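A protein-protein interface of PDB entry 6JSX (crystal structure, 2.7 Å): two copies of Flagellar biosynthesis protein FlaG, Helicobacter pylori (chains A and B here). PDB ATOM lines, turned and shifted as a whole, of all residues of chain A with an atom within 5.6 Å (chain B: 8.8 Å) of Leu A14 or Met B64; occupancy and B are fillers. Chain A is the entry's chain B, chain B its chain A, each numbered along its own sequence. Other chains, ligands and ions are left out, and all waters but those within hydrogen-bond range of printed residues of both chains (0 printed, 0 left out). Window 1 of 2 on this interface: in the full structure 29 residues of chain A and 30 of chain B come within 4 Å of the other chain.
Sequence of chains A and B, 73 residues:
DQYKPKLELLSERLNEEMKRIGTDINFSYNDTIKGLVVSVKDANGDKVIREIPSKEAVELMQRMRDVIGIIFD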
ATOM      1  N   LEU A   9     -13.873  21.561 -34.780  1.00  0.00           N
ATOM      2  CA  LEU A   9     -12.939  20.487 -34.468  1.00  0.00           C
ATOM      3  C   LEU A   9     -12.941  20.228 -32.987  1.00  0.00           C
ATOM      4  O   LEU A   9     -12.932  19.082 -32.540  1.00  0.00           O
ATOM      5  CB  LEU A   9     -11.522  20.848 -34.895  1.00  0.00           C
ATOM      6  CG  LEU A   9     -11.033  20.134 -36.148  1.00  0.00           C
ATOM      7  CD1 LEU A   9     -11.151  18.625 -35.977  1.00  0.00           C
ATOM      8  CD2 LEU A   9     -11.828  20.630 -37.354  1.00  0.00           C
ATOM      9  N   LEU A  10     -12.939  21.306 -32.227  1.00  0.00           N
ATOM     10  CA  LEU A  10     -12.872  21.184 -30.790  1.00  0.00           C
ATOM     11  C   LEU A  10     -14.074  20.412 -30.265  1.00  0.00           C
ATOM     12  O   LEU A  10     -13.903  19.440 -29.526  1.00  0.00           O
ATOM     13  CB  LEU A  10     -12.812  22.554 -30.135  1.00  0.00           C
ATOM     14  CG  LEU A  10     -12.510  22.357 -28.655  1.00  0.00           C
ATOM     15  CD1 LEU A  10     -11.019  22.152 -28.469  1.00  0.00           C
ATOM     16  CD2 LEU A  10     -13.037  23.524 -27.843  1.00  0.00           C
ATOM     17  N   SER A  11     -15.270  20.854 -30.662  1.00  0.00           N
ATOM     18  CA  SER A  11     -16.535  20.234 -30.300  1.00  0.00           C
ATOM     19  C   SER A  11     -16.531  18.760 -30.661  1.00  0.00           C
ATOM     20  O   SER A  11     -16.944  17.912 -29.881  1.00  0.00           O
ATOM     21  CB  SER A  11     -17.681  20.905 -31.059  1.00  0.00           C
ATOM     22  OG  SER A  11     -17.748  22.302 -30.827  1.00  0.00           O
ATOM     23  N   GLU A  12     -16.078  18.468 -31.870  1.00  0.00           N
ATOM     24  CA  GLU A  12     -16.018  17.111 -32.367  1.00  0.00           C
ATOM     25  C   GLU A  12     -15.127  16.245 -31.497  1.00  0.00           C
ATOM     26  O   GLU A  12     -15.526  15.150 -31.076  1.00  0.00           O
ATOM     27  CB  GLU A  12     -15.501  17.125 -33.792  1.00  0.00           C
ATOM     28  CG  GLU A  12     -15.301  15.760 -34.393  1.00  0.00           C
ATOM     29  CD  GLU A  12     -15.104  15.833 -35.897  1.00  0.00           C
ATOM     30  OE1 GLU A  12     -15.372  16.910 -36.481  1.00  0.00           O
ATOM     31  OE2 GLU A  12     -14.688  14.818 -36.496  1.00  0.00           O
ATOM     32  N   ARG A  13     -13.923  16.735 -31.220  1.00  0.00           N
ATOM     33  CA  ARG A  13     -12.973  15.984 -30.404  1.00  0.00           C
ATOM     34  C   ARG A  13     -13.443  15.947 -28.957  1.00  0.00           C
ATOM     35  O   ARG A  13     -13.405  14.902 -28.303  1.00  0.00           O
ATOM     36  CB  ARG A  13     -11.576  16.578 -30.521  1.00  0.00           C
ATOM     37  CG  ARG A  13     -10.959  16.394 -31.908  1.00  0.00           C
ATOM     38  CD  ARG A  13     -10.502  14.954 -32.133  1.00  0.00           C
ATOM     39  NE  ARG A  13     -10.387  14.602 -33.552  1.00  0.00           N
ATOM     40  CZ  ARG A  13     -11.393  14.133 -34.288  1.00  0.00           C
ATOM     41  NH1 ARG A  13     -12.588  13.973 -33.742  1.00  0.00           N
ATOM     42  NH2 ARG A  13     -11.217  13.832 -35.567  1.00  0.00           N
ATOM     43  N   LEU A  14     -13.919  17.080 -28.463  1.00  0.00           N
ATOM     44  CA  LEU A  14     -14.525  17.111 -27.134  1.00  0.00           C
ATOM     45  C   LEU A  14     -15.641  16.075 -26.936  1.00  0.00           C
ATOM     46  O   LEU A  14     -15.712  15.441 -25.889  1.00  0.00           O
ATOM     47  CB  LEU A  14     -15.023  18.516 -26.801  1.00  0.00           C
ATOM     48  CG  LEU A  14     -13.949  19.424 -26.198  1.00  0.00           C
ATOM     49  CD1 LEU A  14     -14.508  20.813 -26.018  1.00  0.00           C
ATOM     50  CD2 LEU A  14     -13.491  18.872 -24.853  1.00  0.00           C
ATOM     51  N   ASN A  15     -16.492  15.904 -27.949  1.00  0.00           N
ATOM     52  CA  ASN A  15     -17.603  14.952 -27.903  1.00  0.00           C
ATOM     53  C   ASN A  15     -17.154  13.490 -27.866  1.00  0.00           C
ATOM     54  O   ASN A  15     -17.706  12.671 -27.118  1.00  0.00           O
ATOM     55  CB  ASN A  15     -18.539  15.174 -29.088  1.00  0.00           C
ATOM     56  CG  ASN A  15     -19.463  16.362 -28.887  1.00  0.00           C
ATOM     57  OD1 ASN A  15     -19.806  16.712 -27.758  1.00  0.00           O
ATOM     58  ND2 ASN A  15     -19.873  16.992 -29.986  1.00  0.00           N
ATOM     59  N   GLU A  16     -16.160  13.161 -28.685  1.00  0.00           N
ATOM     60  CA  GLU A  16     -15.554  11.832 -28.648  1.00  0.00           C
ATOM     61  C   GLU A  16     -15.051  11.541 -27.242  1.00  0.00           C
ATOM     62  O   GLU A  16     -15.257  10.450 -26.713  1.00  0.00           O
ATOM     63  CB  GLU A  16     -14.383  11.746 -29.625  1.00  0.00           C
ATOM     64  CG  GLU A  16     -14.762  11.829 -31.091  1.00  0.00           C
ATOM     65  CD  GLU A  16     -13.563  11.645 -32.003  1.00  0.00           C
ATOM     66  OE1 GLU A  16     -12.413  11.743 -31.511  1.00  0.00           O
ATOM     67  OE2 GLU A  16     -13.766  11.396 -33.212  1.00  0.00           O
ATOM     68  N   GLU A  17     -14.394  12.528 -26.642  1.00  0.00           N
ATOM     69  CA  GLU A  17     -13.869  12.384 -25.291  1.00  0.00           C
ATOM     70  C   GLU A  17     -14.969  12.200 -24.241  1.00  0.00           C
ATOM     71  O   GLU A  17     -14.856  11.345 -23.363  1.00  0.00           O
ATOM     72  CB  GLU A  17     -12.945  13.555 -24.934  1.00  0.00           C
ATOM     73  CG  GLU A  17     -11.579  13.505 -25.625  1.00  0.00           C
ATOM     74  CD  GLU A  17     -10.788  12.238 -25.293  1.00  0.00           C
ATOM     75  OE1 GLU A  17     -11.005  11.667 -24.204  1.00  0.00           O
ATOM     76  OE2 GLU A  17      -9.954  11.806 -26.120  1.00  0.00           O
ATOM     77  N   MET A  18     -16.031  12.992 -24.333  1.00  0.00           N
ATOM     78  CA  MET A  18     -17.135  12.874 -23.385  1.00  0.00           C
ATOM     79  C   MET A  18     -17.779  11.495 -23.502  1.00  0.00           C
ATOM     80  O   MET A  18     -18.089  10.846 -22.496  1.00  0.00           O
ATOM     81  CB  MET A  18     -18.155  13.997 -23.597  1.00  0.00           C
ATOM     82  CG  MET A  18     -17.617  15.373 -23.216  1.00  0.00           C
ATOM     83  SD  MET A  18     -17.205  15.487 -21.484  1.00  0.00           S
ATOM     84  CE  MET A  18     -15.670  16.343 -21.556  1.00  0.00           C
ATOM     85  N   LYS A  19     -17.944  11.044 -24.742  1.00  0.00           N
ATOM     86  CA  LYS A  19     -18.468   9.714 -25.037  1.00  0.00           C
ATOM     87  C   LYS A  19     -17.547   8.609 -24.500  1.00  0.00           C
ATOM     88  O   LYS A  19     -18.011   7.531 -24.160  1.00  0.00           O
ATOM     89  CB  LYS A  19     -18.658   9.561 -26.552  1.00  0.00           C
ATOM     90  CG  LYS A  19     -19.234   8.231 -27.018  1.00  0.00           C
ATOM     91  CD  LYS A  19     -19.476   8.249 -28.522  1.00  0.00           C
ATOM     92  CE  LYS A  19     -20.122   6.953 -29.013  1.00  0.00           C
ATOM     93  NZ  LYS A  19     -20.917   7.156 -30.269  1.00  0.00           N
ATOM     94  N   ILE A  25     -22.287  15.252 -21.913  1.00  0.00           N
ATOM     95  CA  ILE A  25     -22.036  16.670 -22.154  1.00  0.00           C
ATOM     96  C   ILE A  25     -21.813  16.793 -23.649  1.00  0.00           C
ATOM     97  O   ILE A  25     -20.935  16.121 -24.191  1.00  0.00           O
ATOM     98  CB  ILE A  25     -20.807  17.190 -21.358  1.00  0.00           C
ATOM     99  CG1 ILE A  25     -21.019  16.984 -19.848  1.00  0.00           C
ATOM    100  CG2 ILE A  25     -20.526  18.655 -21.666  1.00  0.00           C
ATOM    101  CD1 ILE A  25     -19.941  17.575 -18.966  1.00  0.00           C
ATOM    102  N   PHE A  27     -20.979  19.174 -27.039  1.00  0.00           N
ATOM    103  CA  PHE A  27     -20.363  20.413 -27.508  1.00  0.00           C
ATOM    104  C   PHE A  27     -20.661  20.584 -28.974  1.00  0.00           C
ATOM    105  O   PHE A  27     -20.642  19.607 -29.730  1.00  0.00           O
ATOM    106  CB  PHE A  27     -18.841  20.360 -27.338  1.00  0.00           C
ATOM    107  CG  PHE A  27     -18.388  20.450 -25.909  1.00  0.00           C
ATOM    108  CD1 PHE A  27     -18.130  21.685 -25.333  1.00  0.00           C
ATOM    109  CD2 PHE A  27     -18.231  19.296 -25.138  1.00  0.00           C
ATOM    110  CE1 PHE A  27     -17.727  21.775 -24.013  1.00  0.00           C
ATOM    111  CE2 PHE A  27     -17.819  19.376 -23.816  1.00  0.00           C
ATOM    112  CZ  PHE A  27     -17.565  20.622 -23.249  1.00  0.00           C
ATOM    113  N   MET A  61     -10.439  28.475 -24.250  1.00  0.00           N
ATOM    114  CA  MET A  61      -9.705  27.277 -24.616  1.00  0.00           C
ATOM    115  C   MET A  61      -8.209  27.525 -24.568  1.00  0.00           C
ATOM    116  O   MET A  61      -7.467  26.712 -24.027  1.00  0.00           O
ATOM    117  CB  MET A  61     -10.134  26.788 -25.998  1.00  0.00           C
ATOM    118  CG  MET A  61     -11.507  26.153 -25.978  1.00  0.00           C
ATOM    119  SD  MET A  61     -11.588  24.922 -24.694  1.00  0.00           S
ATOM    120  CE  MET A  61     -13.332  24.791 -24.425  1.00  0.00           C
ATOM    121  N   ILE A  68      -3.712  23.772 -17.659  1.00  0.00           N
ATOM    122  CA  ILE A  68      -3.628  22.320 -17.719  1.00  0.00           C
ATOM    123  C   ILE A  68      -2.159  21.911 -17.856  1.00  0.00           C
ATOM    124  O   ILE A  68      -1.694  20.972 -17.180  1.00  0.00           O
ATOM    125  CB  ILE A  68      -4.435  21.764 -18.900  1.00  0.00           C
ATOM    126  CG1 ILE A  68      -5.932  21.881 -18.631  1.00  0.00           C
ATOM    127  CG2 ILE A  68      -4.078  20.315 -19.151  1.00  0.00           C
ATOM    128  CD1 ILE A  68      -6.795  21.737 -19.883  1.00  0.00           C
ATOM    129  N   ALA B  57     -10.879  12.122 -15.179  1.00  0.00           N
ATOM    130  CA  ALA B  57     -10.830  13.570 -15.338  1.00  0.00           C
ATOM    131  C   ALA B  57      -9.430  14.053 -15.676  1.00  0.00           C
ATOM    132  O   ALA B  57      -9.246  14.973 -16.483  1.00  0.00           O
ATOM    133  CB  ALA B  57     -11.325  14.249 -14.069  1.00  0.00           C
ATOM    134  N   VAL B  58      -8.436  13.439 -15.052  1.00  0.00           N
ATOM    135  CA  VAL B  58      -7.058  13.835 -15.291  1.00  0.00           C
ATOM    136  C   VAL B  58      -6.596  13.418 -16.693  1.00  0.00           C
ATOM    137  O   VAL B  58      -5.911  14.179 -17.384  1.00  0.00           O
ATOM    138  CB  VAL B  58      -6.133  13.282 -14.201  1.00  0.00           C
ATOM    139  CG1 VAL B  58      -4.693  13.714 -14.457  1.00  0.00           C
ATOM    140  CG2 VAL B  58      -6.610  13.756 -12.835  1.00  0.00           C
ATOM    141  N   GLU B  59      -6.989  12.217 -17.112  1.00  0.00           N
ATOM    142  CA  GLU B  59      -6.719  11.752 -18.473  1.00  0.00           C
ATOM    143  C   GLU B  59      -7.369  12.653 -19.521  1.00  0.00           C
ATOM    144  O   GLU B  59      -6.766  12.960 -20.552  1.00  0.00           O
ATOM    145  CB  GLU B  59      -7.196  10.312 -18.654  1.00  0.00           C
ATOM    146  CG  GLU B  59      -6.407   9.304 -17.817  1.00  0.00           C
ATOM    147  CD  GLU B  59      -6.961   7.885 -17.898  1.00  0.00           C
ATOM    148  OE1 GLU B  59      -8.067   7.692 -18.464  1.00  0.00           O
ATOM    149  OE2 GLU B  59      -6.280   6.966 -17.388  1.00  0.00           O
ATOM    150  N   LEU B  60      -8.595  13.078 -19.236  1.00  0.00           N
ATOM    151  CA  LEU B  60      -9.383  13.915 -20.137  1.00  0.00           C
ATOM    152  C   LEU B  60      -8.792  15.299 -20.290  1.00  0.00           C
ATOM    153  O   LEU B  60      -8.655  15.803 -21.400  1.00  0.00           O
ATOM    154  CB  LEU B  60     -10.802  14.039 -19.597  1.00  0.00           C
ATOM    155  CG  LEU B  60     -11.693  15.095 -20.217  1.00  0.00           C
ATOM    156  CD1 LEU B  60     -12.121  14.646 -21.592  1.00  0.00           C
ATOM    157  CD2 LEU B  60     -12.883  15.320 -19.313  1.00  0.00           C
ATOM    158  N   MET B  61      -8.459  15.924 -19.168  1.00  0.00           N
ATOM    159  CA  MET B  61      -7.754  17.200 -19.203  1.00  0.00           C
ATOM    160  C   MET B  61      -6.424  17.121 -19.953  1.00  0.00           C
ATOM    161  O   MET B  61      -6.020  18.074 -20.613  1.00  0.00           O
ATOM    162  CB  MET B  61      -7.584  17.765 -17.791  1.00  0.00           C
ATOM    163  CG  MET B  61      -8.911  18.199 -17.168  1.00  0.00           C
ATOM    164  SD  MET B  61      -9.647  19.582 -18.041  1.00  0.00           S
ATOM    165  CE  MET B  61     -10.759  18.806 -19.222  1.00  0.00           C
ATOM    166  N   GLN B  62      -5.759  15.977 -19.890  1.00  0.00           N
ATOM    167  CA  GLN B  62      -4.536  15.810 -20.662  1.00  0.00           C
ATOM    168  C   GLN B  62      -4.769  15.679 -22.175  1.00  0.00           C
ATOM    169  O   GLN B  62      -4.089  16.349 -22.968  1.00  0.00           O
ATOM    170  CB  GLN B  62      -3.679  14.677 -20.103  1.00  0.00           C
ATOM    171  CG  GLN B  62      -2.941  15.094 -18.845  1.00  0.00           C
ATOM    172  CD  GLN B  62      -2.307  13.930 -18.113  1.00  0.00           C
ATOM    173  OE1 GLN B  62      -2.718  12.776 -18.268  1.00  0.00           O
ATOM    174  NE2 GLN B  62      -1.290  14.226 -17.305  1.00  0.00           N
ATOM    175  N   ARG B  63      -5.735  14.845 -22.570  1.00  0.00           N
ATOM    176  CA  ARG B  63      -6.076  14.684 -23.986  1.00  0.00           C
ATOM    177  C   ARG B  63      -6.605  15.991 -24.577  1.00  0.00           C
ATOM    178  O   ARG B  63      -6.393  16.295 -25.756  1.00  0.00           O
ATOM    179  CB  ARG B  63      -7.096  13.560 -24.193  1.00  0.00           C
ATOM    180  CG  ARG B  63      -6.671  12.205 -23.616  1.00  0.00           C
ATOM    181  CD  ARG B  63      -7.741  11.129 -23.846  1.00  0.00           C
ATOM    182  NE  ARG B  63      -7.565   9.958 -22.987  1.00  0.00           N
ATOM    183  CZ  ARG B  63      -8.404   9.597 -22.016  1.00  0.00           C
ATOM    184  NH1 ARG B  63      -9.500  10.305 -21.774  1.00  0.00           N
ATOM    185  NH2 ARG B  63      -8.149   8.513 -21.290  1.00  0.00           N
ATOM    186  N   MET B  64      -7.283  16.783 -23.759  1.00  0.00           N
ATOM    187  CA  MET B  64      -7.736  18.066 -24.254  1.00  0.00           C
ATOM    188  C   MET B  64      -6.582  19.062 -24.401  1.00  0.00           C
ATOM    189  O   MET B  64      -6.616  19.921 -25.283  1.00  0.00           O
ATOM    190  CB  MET B  64      -8.913  18.615 -23.436  1.00  0.00           C
ATOM    191  CG  MET B  64     -10.203  17.829 -23.672  1.00  0.00           C
ATOM    192  SD  MET B  64     -10.298  17.055 -25.327  1.00  0.00           S
ATOM    193  CE  MET B  64     -10.460  18.493 -26.390  1.00  0.00           C
ATOM    194  N   ARG B  65      -5.554  18.928 -23.569  1.00  0.00           N
ATOM    195  CA  ARG B  65      -4.397  19.811 -23.679  1.00  0.00           C
ATOM    196  C   ARG B  65      -3.745  19.725 -25.060  1.00  0.00           C
ATOM    197  O   ARG B  65      -3.433  20.745 -25.680  1.00  0.00           O
ATOM    198  CB  ARG B  65      -3.355  19.508 -22.600  1.00  0.00           C
ATOM    199  CG  ARG B  65      -1.993  20.106 -22.920  1.00  0.00           C
ATOM    200  CD  ARG B  65      -1.106  20.261 -21.704  1.00  0.00           C
ATOM    201  NE  ARG B  65      -0.110  21.309 -21.924  1.00  0.00           N
ATOM    202  CZ  ARG B  65       1.142  21.090 -22.315  1.00  0.00           C
ATOM    203  NH1 ARG B  65       1.573  19.850 -22.516  1.00  0.00           N
ATOM    204  NH2 ARG B  65       1.969  22.115 -22.493  1.00  0.00           N
ATOM    205  N   ASP B  66      -3.550  18.503 -25.537  1.00  0.00           N
ATOM    206  CA  ASP B  66      -2.920  18.279 -26.830  1.00  0.00           C
ATOM    207  C   ASP B  66      -3.839  18.578 -28.011  1.00  0.00           C
ATOM    208  O   ASP B  66      -3.380  19.019 -29.060  1.00  0.00           O
ATOM    209  CB  ASP B  66      -2.398  16.855 -26.898  1.00  0.00           C
ATOM    210  CG  ASP B  66      -1.473  16.540 -25.751  1.00  0.00           C
ATOM    211  OD1 ASP B  66      -0.292  16.959 -25.816  1.00  0.00           O
ATOM    212  OD2 ASP B  66      -1.936  15.899 -24.778  1.00  0.00           O
ATOM    213  N   VAL B  67      -5.132  18.337 -27.849  1.00  0.00           N
ATOM    214  CA  VAL B  67      -6.082  18.702 -28.887  1.00  0.00           C
ATOM    215  C   VAL B  67      -6.093  20.218 -29.029  1.00  0.00           C
ATOM    216  O   VAL B  67      -5.953  20.747 -30.131  1.00  0.00           O
ATOM    217  CB  VAL B  67      -7.488  18.170 -28.582  1.00  0.00           C
ATOM    218  CG1 VAL B  67      -8.523  18.846 -29.468  1.00  0.00           C
ATOM    219  CG2 VAL B  67      -7.521  16.661 -28.762  1.00  0.00           C
ATOM    220  N   ILE B  68      -6.222  20.910 -27.900  1.00  0.00           N
ATOM    221  CA  ILE B  68      -6.171  22.374 -27.869  1.00  0.00           C
ATOM    222  C   ILE B  68      -4.843  22.924 -28.418  1.00  0.00           C
ATOM    223  O   ILE B  68      -4.797  23.987 -29.044  1.00  0.00           O
ATOM    224  CB  ILE B  68      -6.453  22.909 -26.443  1.00  0.00           C
ATOM    225  CG1 ILE B  68      -7.904  22.614 -26.051  1.00  0.00           C
ATOM    226  CG2 ILE B  68      -6.216  24.394 -26.362  1.00  0.00           C
ATOM    227  CD1 ILE B  68      -8.281  23.088 -24.657  1.00  0.00           C
ATOM    228  N   GLY B  69      -3.767  22.183 -28.206  1.00  0.00           N
ATOM    229  CA  GLY B  69      -2.483  22.572 -28.743  1.00  0.00           C
ATOM    230  C   GLY B  69      -2.513  22.615 -30.253  1.00  0.00           C
ATOM    231  O   GLY B  69      -2.244  23.655 -30.846  1.00  0.00           O
ATOM    232  N   ILE B  70      -2.855  21.491 -30.879  1.00  0.00           N
ATOM    233  CA  ILE B  70      -2.826  21.382 -32.341  1.00  0.00           C
ATOM    234  C   ILE B  70      -3.872  22.288 -33.010  1.00  0.00           C
ATOM    235  O   ILE B  70      -3.634  22.859 -34.079  1.00  0.00           O
ATOM    236  CB  ILE B  70      -2.991  19.913 -32.804  1.00  0.00           C
ATOM    237  CG1 ILE B  70      -1.792  19.085 -32.353  1.00  0.00           C
ATOM    238  CG2 ILE B  70      -3.103  19.823 -34.315  1.00  0.00           C
ATOM    239  CD1 ILE B  70      -0.483  19.559 -32.947  1.00  0.00           C
ATOM    240  N   ILE B  71      -5.022  22.439 -32.365  1.00  0.00           N
ATOM    241  CA  ILE B  71      -6.044  23.321 -32.889  1.00  0.00           C
ATOM    242  C   ILE B  71      -5.701  24.811 -32.747  1.00  0.00           C
ATOM    243  O   ILE B  71      -5.911  25.571 -33.689  1.00  0.00           O
ATOM    244  CB  ILE B  71      -7.431  23.020 -32.277  1.00  0.00           C
ATOM    245  CG1 ILE B  71      -7.824  21.561 -32.519  1.00  0.00           C
ATOM    246  CG2 ILE B  71      -8.489  23.914 -32.881  1.00  0.00           C
ATOM    247  CD1 ILE B  71      -9.224  21.212 -32.030  1.00  0.00           C
ATOM    248  N   PHE B  72      -5.167  25.237 -31.600  1.00  0.00           N
ATOM    249  CA  PHE B  72      -4.989  26.681 -31.359  1.00  0.00           C
ATOM    250  C   PHE B  72      -3.559  27.205 -31.191  1.00  0.00           C
ATOM    251  O   PHE B  72      -3.368  28.402 -30.961  1.00  0.00           O
ATOM    252  CB  PHE B  72      -5.811  27.141 -30.153  1.00  0.00           C
ATOM    253  CG  PHE B  72      -7.261  26.776 -30.229  1.00  0.00           C
ATOM    254  CD1 PHE B  72      -8.155  27.576 -30.922  1.00  0.00           C
ATOM    255  CD2 PHE B  72      -7.738  25.634 -29.595  1.00  0.00           C
ATOM    256  CE1 PHE B  72      -9.506  27.235 -30.995  1.00  0.00           C
ATOM    257  CE2 PHE B  72      -9.091  25.284 -29.659  1.00  0.00           C
ATOM    258  CZ  PHE B  72      -9.974  26.089 -30.363  1.00  0.00           C
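The side-chain carboxylate (OE1) of Glu A17 lies within salt-bridge range of the guanidinium group (NH1) of Arg B63.
The side-chain carboxylate of Glu B59 lies within salt-bridge range of the guanidinium group of Arg B63 (2.9 Å). The side-chain carboxylate of Glu A12 lies within salt-bridge range of the guanidinium group of Arg A13 (3.6 Å). OE2 of Glu A16 lies within salt-bridge range of NH1 of Arg A13, 2.9 Å away.
Among the printed residues, merely in contact across the chains: Ile A68 with Met B61 (3.3 Å), Leu A14 with Met B64 (3.4 Å), Met A61 with Ile B68 (3.5 Å), Glu A17 with Leu B60 (3.6 Å), Ile A68 with Arg B65 (3.6 Å), Leu A9 with Ile B71 (3.7 Å), Met A18 with Leu B60 (3.7 Å), Leu A10 with Ile B71 (3.7 Å), Glu A17 with Met B64 (3.8 Å), Leu A10 with Phe B72 (3.9 Å), Arg A13 with Val B67 (3.9 Å) and Leu A10 with Ile B68 (3.97 Å).
Printed residues of chain B within 4 Å of Leu A14: Met B64 (3.4 Å). Met B64 touches just these residues of chain A: Leu A14 (3.4 Å) and Glu A17 (3.8 Å). Of the printed residues of chain B, Glu A17 touches Leu B60, Arg B63 and Met B64. Printed residues of chain B within 4 Å of Met A18: Leu B60. Of the printed residues of chain A, Arg B63 touches Glu A17 (3.2 Å). Of the printed residues of chain A, Phe B72 touches Leu A10. Printed residues of chain B within 4 Å of Met A61: Ile B68. Ile A25 touches none of the printed residues of chain B. Val B58 touches none of the printed residues of chain A. The nearest residue of chain B that does not touch Leu A14 is Leu B60 (5.5 Å).
Printed residues of chain A that touch a printed residue of chain B: Leu A9, Leu A10, Arg A13, Leu A14, Glu A17, Met A18, Met A61 and Ile A68. Hydrophobic or aromatic side chains of chain A within 4 Å of the printed part of chain B: Leu A9, Leu A10, Leu A14, Met A18, Met A61 and Ile A68. Hydrophobic or aromatic side chains of chain B that line the printed part of chain A: Leu B60, Met B64, Val B67, Ile B68, Ile B71 and Phe B72. Among the printed residues, Asp or Glu carboxylates within 4 Å of a Lys or Arg side-chain nitrogen of the other chain: Glu A17 with Arg B63.
Met A61 touches Ile B68, and with the chains exchanged Ile A68 touches Met B61. Positions printed for both chains: 61 and 68. Of the 13 pairs that touch across the chains among the printed residues, 2 have their exchanged pair printed and touching as well.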
